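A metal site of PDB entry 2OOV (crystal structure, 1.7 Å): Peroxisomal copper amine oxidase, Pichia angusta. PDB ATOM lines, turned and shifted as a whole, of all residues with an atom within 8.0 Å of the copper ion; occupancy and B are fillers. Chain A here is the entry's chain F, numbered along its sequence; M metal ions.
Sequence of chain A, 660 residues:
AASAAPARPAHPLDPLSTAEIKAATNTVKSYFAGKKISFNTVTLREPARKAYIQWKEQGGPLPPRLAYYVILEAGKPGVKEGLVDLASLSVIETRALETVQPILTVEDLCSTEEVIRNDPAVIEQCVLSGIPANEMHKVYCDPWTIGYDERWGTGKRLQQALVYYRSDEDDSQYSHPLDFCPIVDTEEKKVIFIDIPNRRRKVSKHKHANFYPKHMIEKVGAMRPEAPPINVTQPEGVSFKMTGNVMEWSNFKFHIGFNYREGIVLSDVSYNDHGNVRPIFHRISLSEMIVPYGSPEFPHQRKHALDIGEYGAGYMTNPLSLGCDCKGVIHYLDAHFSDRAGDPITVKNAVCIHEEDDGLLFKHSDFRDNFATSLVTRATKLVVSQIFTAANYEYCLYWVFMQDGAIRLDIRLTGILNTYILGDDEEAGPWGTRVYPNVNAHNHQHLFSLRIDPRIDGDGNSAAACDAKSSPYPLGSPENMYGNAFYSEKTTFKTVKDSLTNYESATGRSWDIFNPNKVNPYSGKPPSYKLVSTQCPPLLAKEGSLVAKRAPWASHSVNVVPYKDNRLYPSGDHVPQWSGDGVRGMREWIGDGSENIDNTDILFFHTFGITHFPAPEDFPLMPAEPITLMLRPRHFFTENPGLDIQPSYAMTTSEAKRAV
A ring nitrogen (NE2) of His 612 is in hydrogen-bond range of the side-chain carboxylate (OD2) of Asp 618, 2.9 Å away. N of His 446 lies within hydrogen-bond range of O of Ile 610 (2.9 Å). The side-chain hydroxyl of Tyr 395 lies within hydrogen-bond range of a ring nitrogen (ND1) of His 446 (2.8 Å). ND1 of His 444 sits at hydrogen-bond distance from O of His 442 (3.0 Å).
Of the 23 residues printed, 3 come within 4 Å of the copper ion.
A ring nitrogen (ND1) of His 612 is bound to the copper ion (2.0 Å). NE2 of His 446 is bound to the copper ion (2.0 Å). NE2 of His 444 binds the copper ion (2.0 Å). The copper ion has three donor atoms within binding distance.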
ATOM      1  N   VAL A 291      23.903 -14.641  21.734  1.00  0.00           N
ATOM      2  CA  VAL A 291      23.674 -15.680  20.724  1.00  0.00           C
ATOM      3  C   VAL A 291      23.026 -16.912  21.410  1.00  0.00           C
ATOM      4  O   VAL A 291      23.690 -17.934  21.644  1.00  0.00           O
ATOM      5  CB  VAL A 291      25.001 -16.014  19.968  1.00  0.00           C
ATOM      6  CG1 VAL A 291      24.794 -17.087  18.862  1.00  0.00           C
ATOM      7  CG2 VAL A 291      25.610 -14.741  19.346  1.00  0.00           C
ATOM      8  N   TYR A 293      21.267 -20.234  22.165  1.00  0.00           N
ATOM      9  CA  TYR A 293      20.916 -21.524  21.543  1.00  0.00           C
ATOM     10  C   TYR A 293      19.575 -22.040  22.060  1.00  0.00           C
ATOM     11  O   TYR A 293      19.117 -21.675  23.160  1.00  0.00           O
ATOM     12  CB  TYR A 293      22.072 -22.549  21.672  1.00  0.00           C
ATOM     13  CG  TYR A 293      23.111 -22.280  20.612  1.00  0.00           C
ATOM     14  CD1 TYR A 293      23.984 -21.186  20.733  1.00  0.00           C
ATOM     15  CD2 TYR A 293      23.209 -23.082  19.479  1.00  0.00           C
ATOM     16  CE1 TYR A 293      24.918 -20.897  19.748  1.00  0.00           C
ATOM     17  CE2 TYR A 293      24.144 -22.800  18.461  1.00  0.00           C
ATOM     18  CZ  TYR A 293      24.985 -21.687  18.608  1.00  0.00           C
ATOM     19  OH  TYR A 293      25.907 -21.376  17.639  1.00  0.00           O
ATOM     20  N   ASN A 392      34.133 -20.593  16.309  1.00  0.00           N
ATOM     21  CA  ASN A 392      33.584 -21.099  15.030  1.00  0.00           C
ATOM     22  C   ASN A 392      33.059 -20.010  14.085  1.00  0.00           C
ATOM     23  O   ASN A 392      33.145 -20.176  12.849  1.00  0.00           O
ATOM     24  CB  ASN A 392      32.495 -22.162  15.267  1.00  0.00           C
ATOM     25  CG  ASN A 392      31.396 -21.661  16.185  1.00  0.00           C
ATOM     26  OD1 ASN A 392      31.632 -21.373  17.358  1.00  0.00           O
ATOM     27  ND2 ASN A 392      30.182 -21.540  15.648  1.00  0.00           N
ATOM     28  N   TPQ A 393      32.548 -18.936  14.550  1.00  0.00           N
ATOM     29  CA  TPQ A 393      31.788 -17.897  13.833  1.00  0.00           C
ATOM     30  CB  TPQ A 393      30.855 -17.100  14.738  1.00  0.00           C
ATOM     31  C   TPQ A 393      32.723 -16.859  13.275  1.00  0.00           C
ATOM     32  O   TPQ A 393      33.611 -16.450  14.067  1.00  0.00           O
ATOM     33  C1  TPQ A 393      30.071 -17.951  15.701  1.00  0.00           C
ATOM     34  C2  TPQ A 393      28.754 -18.492  15.299  1.00  0.00           C
ATOM     35  O2  TPQ A 393      28.271 -18.224  14.055  1.00  0.00           O
ATOM     36  C3  TPQ A 393      28.005 -19.255  16.180  1.00  0.00           C
ATOM     37  C4  TPQ A 393      28.537 -19.503  17.430  1.00  0.00           C
ATOM     38  O4  TPQ A 393      27.854 -20.229  18.328  1.00  0.00           O
ATOM     39  C5  TPQ A 393      29.847 -18.963  17.849  1.00  0.00           C
ATOM     40  O5  TPQ A 393      30.321 -19.229  19.095  1.00  0.00           O
ATOM     41  C6  TPQ A 393      30.581 -18.182  16.975  1.00  0.00           C
ATOM     42  N   TYR A 395      32.077 -12.698  12.264  1.00  0.00           N
ATOM     43  CA  TYR A 395      31.154 -11.569  12.163  1.00  0.00           C
ATOM     44  C   TYR A 395      31.811 -10.457  11.370  1.00  0.00           C
ATOM     45  O   TYR A 395      32.817  -9.918  11.804  1.00  0.00           O
ATOM     46  CB  TYR A 395      30.803 -11.050  13.559  1.00  0.00           C
ATOM     47  CG  TYR A 395      29.937 -12.017  14.340  1.00  0.00           C
ATOM     48  CD1 TYR A 395      30.514 -13.037  15.112  1.00  0.00           C
ATOM     49  CD2 TYR A 395      28.547 -11.949  14.285  1.00  0.00           C
ATOM     50  CE1 TYR A 395      29.728 -13.954  15.815  1.00  0.00           C
ATOM     51  CE2 TYR A 395      27.740 -12.857  14.979  1.00  0.00           C
ATOM     52  CZ  TYR A 395      28.332 -13.848  15.743  1.00  0.00           C
ATOM     53  OH  TYR A 395      27.554 -14.755  16.425  1.00  0.00           O
ATOM     54  N   LEU A 413      27.235 -12.668   8.456  1.00  0.00           N
ATOM     55  CA  LEU A 413      27.637 -13.769   9.334  1.00  0.00           C
ATOM     56  C   LEU A 413      28.173 -14.870   8.459  1.00  0.00           C
ATOM     57  O   LEU A 413      27.512 -15.274   7.500  1.00  0.00           O
ATOM     58  CB  LEU A 413      26.450 -14.328  10.113  1.00  0.00           C
ATOM     59  CG  LEU A 413      25.547 -13.363  10.872  1.00  0.00           C
ATOM     60  CD1 LEU A 413      24.512 -14.121  11.700  1.00  0.00           C
ATOM     61  CD2 LEU A 413      26.353 -12.432  11.754  1.00  0.00           C
ATOM     62  N   THR A 414      29.359 -15.370   8.789  1.00  0.00           N
ATOM     63  CA  THR A 414      29.888 -16.542   8.095  1.00  0.00           C
ATOM     64  C   THR A 414      30.662 -17.385   9.119  1.00  0.00           C
ATOM     65  O   THR A 414      30.404 -17.287  10.322  1.00  0.00           O
ATOM     66  CB  THR A 414      30.678 -16.151   6.789  1.00  0.00           C
ATOM     67  OG1 THR A 414      31.158 -17.341   6.135  1.00  0.00           O
ATOM     68  CG2 THR A 414      31.843 -15.235   7.087  1.00  0.00           C
ATOM     69  N   ILE A 416      31.534 -21.119  10.690  1.00  0.00           N
ATOM     70  CA  ILE A 416      31.135 -22.518  10.806  1.00  0.00           C
ATOM     71  C   ILE A 416      30.065 -22.627  11.876  1.00  0.00           C
ATOM     72  O   ILE A 416      30.132 -21.976  12.922  1.00  0.00           O
ATOM     73  CB  ILE A 416      32.361 -23.390  11.160  1.00  0.00           C
ATOM     74  CG1 ILE A 416      33.430 -23.284  10.044  1.00  0.00           C
ATOM     75  CG2 ILE A 416      31.953 -24.849  11.393  1.00  0.00           C
ATOM     76  CD1 ILE A 416      34.692 -24.035  10.335  1.00  0.00           C
ATOM     77  N   LEU A 417      29.048 -23.443  11.603  1.00  0.00           N
ATOM     78  CA  LEU A 417      28.042 -23.775  12.601  1.00  0.00           C
ATOM     79  C   LEU A 417      28.643 -24.355  13.870  1.00  0.00           C
ATOM     80  O   LEU A 417      29.558 -25.189  13.796  1.00  0.00           O
ATOM     81  CB  LEU A 417      27.089 -24.822  12.034  1.00  0.00           C
ATOM     82  CG  LEU A 417      26.167 -24.412  10.887  1.00  0.00           C
ATOM     83  CD1 LEU A 417      25.527 -25.668  10.304  1.00  0.00           C
ATOM     84  CD2 LEU A 417      25.129 -23.434  11.415  1.00  0.00           C
ATOM     85  N   ASN A 418      28.111 -23.960  15.028  1.00  0.00           N
ATOM     86  CA  ASN A 418      28.367 -24.705  16.259  1.00  0.00           C
ATOM     87  C   ASN A 418      27.657 -26.051  16.116  1.00  0.00           C
ATOM     88  O   ASN A 418      26.491 -26.087  15.679  1.00  0.00           O
ATOM     89  CB  ASN A 418      27.844 -23.966  17.496  1.00  0.00           C
ATOM     90  CG  ASN A 418      27.664 -24.904  18.701  1.00  0.00           C
ATOM     91  OD1 ASN A 418      26.569 -25.408  18.944  1.00  0.00           O
ATOM     92  ND2 ASN A 418      28.738 -25.127  19.435  1.00  0.00           N
ATOM     93  N   HIS A 442      22.459 -27.037  16.364  1.00  0.00           N
ATOM     94  CA  HIS A 442      21.329 -26.537  17.150  1.00  0.00           C
ATOM     95  C   HIS A 442      20.819 -25.171  16.658  1.00  0.00           C
ATOM     96  O   HIS A 442      21.601 -24.326  16.196  1.00  0.00           O
ATOM     97  CB  HIS A 442      21.742 -26.361  18.614  1.00  0.00           C
ATOM     98  CG  HIS A 442      21.927 -27.628  19.374  1.00  0.00           C
ATOM     99  ND1 HIS A 442      22.833 -27.743  20.409  1.00  0.00           N
ATOM    100  CD2 HIS A 442      21.316 -28.834  19.275  1.00  0.00           C
ATOM    101  CE1 HIS A 442      22.773 -28.959  20.922  1.00  0.00           C
ATOM    102  NE2 HIS A 442      21.873 -29.648  20.244  1.00  0.00           N
ATOM    103  N   ASN A 443      19.507 -24.962  16.787  1.00  0.00           N
ATOM    104  CA  ASN A 443      18.885 -23.646  16.551  1.00  0.00           C
ATOM    105  C   ASN A 443      19.463 -22.571  17.475  1.00  0.00           C
ATOM    106  O   ASN A 443      19.822 -22.866  18.624  1.00  0.00           O
ATOM    107  CB  ASN A 443      17.380 -23.719  16.836  1.00  0.00           C
ATOM    108  CG  ASN A 443      16.653 -24.736  15.983  1.00  0.00           C
ATOM    109  OD1 ASN A 443      17.151 -25.171  14.952  1.00  0.00           O
ATOM    110  ND2 ASN A 443      15.442 -25.096  16.395  1.00  0.00           N
ATOM    111  N   HIS A 444      19.526 -21.335  16.998  1.00  0.00           N
ATOM    112  CA  HIS A 444      20.061 -20.225  17.790  1.00  0.00           C
ATOM    113  C   HIS A 444      19.666 -18.892  17.143  1.00  0.00           C
ATOM    114  O   HIS A 444      19.350 -18.853  15.958  1.00  0.00           O
ATOM    115  CB  HIS A 444      21.603 -20.335  17.906  1.00  0.00           C
ATOM    116  CG  HIS A 444      22.305 -20.353  16.572  1.00  0.00           C
ATOM    117  ND1 HIS A 444      22.357 -21.478  15.778  1.00  0.00           N
ATOM    118  CD2 HIS A 444      22.944 -19.372  15.890  1.00  0.00           C
ATOM    119  CE1 HIS A 444      22.996 -21.178  14.645  1.00  0.00           C
ATOM    120  NE2 HIS A 444      23.357 -19.912  14.696  1.00  0.00           N
ATOM    121  N   GLN A 445      19.693 -17.832  17.942  1.00  0.00           N
ATOM    122  CA  GLN A 445      19.525 -16.474  17.426  1.00  0.00           C
ATOM    123  C   GLN A 445      20.859 -15.757  17.530  1.00  0.00           C
ATOM    124  O   GLN A 445      21.670 -16.103  18.400  1.00  0.00           O
ATOM    125  CB  GLN A 445      18.479 -15.711  18.247  1.00  0.00           C
ATOM    126  CG  GLN A 445      17.127 -16.400  18.312  1.00  0.00           C
ATOM    127  CD  GLN A 445      16.093 -15.516  18.960  1.00  0.00           C
ATOM    128  OE1 GLN A 445      16.022 -15.428  20.206  1.00  0.00           O
ATOM    129  NE2 GLN A 445      15.292 -14.843  18.141  1.00  0.00           N
ATOM    130  N   HIS A 446      21.085 -14.782  16.668  1.00  0.00           N
ATOM    131  CA  HIS A 446      22.220 -13.866  16.835  1.00  0.00           C
ATOM    132  C   HIS A 446      21.580 -12.503  17.067  1.00  0.00           C
ATOM    133  O   HIS A 446      20.873 -12.005  16.162  1.00  0.00           O
ATOM    134  CB  HIS A 446      23.094 -13.786  15.590  1.00  0.00           C
ATOM    135  CG  HIS A 446      23.683 -15.092  15.122  1.00  0.00           C
ATOM    136  ND1 HIS A 446      24.996 -15.455  15.393  1.00  0.00           N
ATOM    137  CD2 HIS A 446      23.191 -16.069  14.328  1.00  0.00           C
ATOM    138  CE1 HIS A 446      25.248 -16.618  14.819  1.00  0.00           C
ATOM    139  NE2 HIS A 446      24.184 -16.997  14.145  1.00  0.00           N
ATOM    140  N   ILE A 610      19.116 -11.974  13.774  1.00  0.00           N
ATOM    141  CA  ILE A 610      18.443 -13.057  13.041  1.00  0.00           C
ATOM    142  C   ILE A 610      18.156 -14.284  13.915  1.00  0.00           C
ATOM    143  O   ILE A 610      18.729 -14.456  14.981  1.00  0.00           O
ATOM    144  CB  ILE A 610      19.238 -13.514  11.809  1.00  0.00           C
ATOM    145  CG1 ILE A 610      20.569 -14.154  12.229  1.00  0.00           C
ATOM    146  CG2 ILE A 610      19.441 -12.343  10.818  1.00  0.00           C
ATOM    147  CD1 ILE A 610      21.106 -15.185  11.235  1.00  0.00           C
ATOM    148  N   THR A 611      17.278 -15.147  13.426  1.00  0.00           N
ATOM    149  CA  THR A 611      16.996 -16.423  14.051  1.00  0.00           C
ATOM    150  C   THR A 611      17.457 -17.487  13.041  1.00  0.00           C
ATOM    151  O   THR A 611      17.000 -17.509  11.904  1.00  0.00           O
ATOM    152  CB  THR A 611      15.502 -16.545  14.393  1.00  0.00           C
ATOM    153  OG1 THR A 611      15.154 -15.525  15.349  1.00  0.00           O
ATOM    154  CG2 THR A 611      15.183 -17.917  14.963  1.00  0.00           C
ATOM    155  N   HIS A 612      18.390 -18.323  13.459  1.00  0.00           N
ATOM    156  CA  HIS A 612      19.082 -19.224  12.542  1.00  0.00           C
ATOM    157  C   HIS A 612      18.586 -20.645  12.763  1.00  0.00           C
ATOM    158  O   HIS A 612      18.796 -21.218  13.838  1.00  0.00           O
ATOM    159  CB  HIS A 612      20.591 -19.120  12.784  1.00  0.00           C
ATOM    160  CG  HIS A 612      21.432 -19.843  11.767  1.00  0.00           C
ATOM    161  ND1 HIS A 612      22.800 -19.750  11.734  1.00  0.00           N
ATOM    162  CD2 HIS A 612      21.082 -20.670  10.738  1.00  0.00           C
ATOM    163  CE1 HIS A 612      23.273 -20.506  10.761  1.00  0.00           C
ATOM    164  NE2 HIS A 612      22.249 -21.062  10.130  1.00  0.00           N
ATOM    165  N   PHE A 613      17.933 -21.220  11.747  1.00  0.00           N
ATOM    166  CA  PHE A 613      17.584 -22.632  11.769  1.00  0.00           C
ATOM    167  C   PHE A 613      18.485 -23.327  10.752  1.00  0.00           C
ATOM    168  O   PHE A 613      18.253 -23.222   9.538  1.00  0.00           O
ATOM    169  CB  PHE A 613      16.116 -22.837  11.399  1.00  0.00           C
ATOM    170  CG  PHE A 613      15.165 -22.224  12.382  1.00  0.00           C
ATOM    171  CD1 PHE A 613      14.877 -22.874  13.583  1.00  0.00           C
ATOM    172  CD2 PHE A 613      14.550 -21.013  12.104  1.00  0.00           C
ATOM    173  CE1 PHE A 613      13.986 -22.311  14.511  1.00  0.00           C
ATOM    174  CE2 PHE A 613      13.663 -20.429  13.031  1.00  0.00           C
ATOM    175  CZ  PHE A 613      13.385 -21.081  14.229  1.00  0.00           C
ATOM    176  N   PRO A 614      19.552 -23.987  11.243  1.00  0.00           N
ATOM    177  CA  PRO A 614      20.540 -24.482  10.292  1.00  0.00           C
ATOM    178  C   PRO A 614      19.979 -25.413   9.239  1.00  0.00           C
ATOM    179  O   PRO A 614      18.979 -26.111   9.466  1.00  0.00           O
ATOM    180  CB  PRO A 614      21.558 -25.207  11.189  1.00  0.00           C
ATOM    181  CG  PRO A 614      21.435 -24.446  12.531  1.00  0.00           C
ATOM    182  CD  PRO A 614      19.930 -24.263  12.635  1.00  0.00           C
ATOM    183  N   ASP A 618      24.483 -24.644   5.021  1.00  0.00           N
ATOM    184  CA  ASP A 618      25.333 -23.899   5.972  1.00  0.00           C
ATOM    185  C   ASP A 618      26.627 -24.634   6.337  1.00  0.00           C
ATOM    186  O   ASP A 618      27.486 -24.073   7.025  1.00  0.00           O
ATOM    187  CB  ASP A 618      24.554 -23.648   7.271  1.00  0.00           C
ATOM    188  CG  ASP A 618      23.315 -22.772   7.084  1.00  0.00           C
ATOM    189  OD1 ASP A 618      23.267 -21.996   6.117  1.00  0.00           O
ATOM    190  OD2 ASP A 618      22.398 -22.867   7.927  1.00  0.00           O
ATOM    191  N   MET A 622      29.733 -21.848   6.191  1.00  0.00           N
ATOM    192  CA  MET A 622      28.466 -21.171   5.870  1.00  0.00           C
ATOM    193  C   MET A 622      28.583 -19.988   4.903  1.00  0.00           C
ATOM    194  O   MET A 622      29.381 -19.094   5.144  1.00  0.00           O
ATOM    195  CB  MET A 622      27.782 -20.692   7.146  1.00  0.00           C
ATOM    196  CG  MET A 622      26.352 -20.214   6.928  1.00  0.00           C
ATOM    197  SD  MET A 622      25.580 -19.743   8.477  1.00  0.00           S
ATOM    198  CE  MET A 622      26.478 -18.225   8.842  1.00  0.00           C
ATOM    199  N   GLU A 625      25.467 -14.597   5.541  1.00  0.00           N
ATOM    200  CA  GLU A 625      24.086 -14.222   5.786  1.00  0.00           C
ATOM    201  C   GLU A 625      24.043 -12.742   6.190  1.00  0.00           C
ATOM    202  O   GLU A 625      24.706 -12.342   7.163  1.00  0.00           O
ATOM    203  CB  GLU A 625      23.439 -15.078   6.892  1.00  0.00           C
ATOM    204  CG  GLU A 625      22.000 -14.652   7.154  1.00  0.00           C
ATOM    205  CD  GLU A 625      21.139 -15.715   7.828  1.00  0.00           C
ATOM    206  OE1 GLU A 625      21.662 -16.758   8.301  1.00  0.00           O
ATOM    207  OE2 GLU A 625      19.917 -15.484   7.913  1.00  0.00           O
HETATM  208 CU    CU M   1      23.761 -18.689  13.143  1.00  0.00          CU
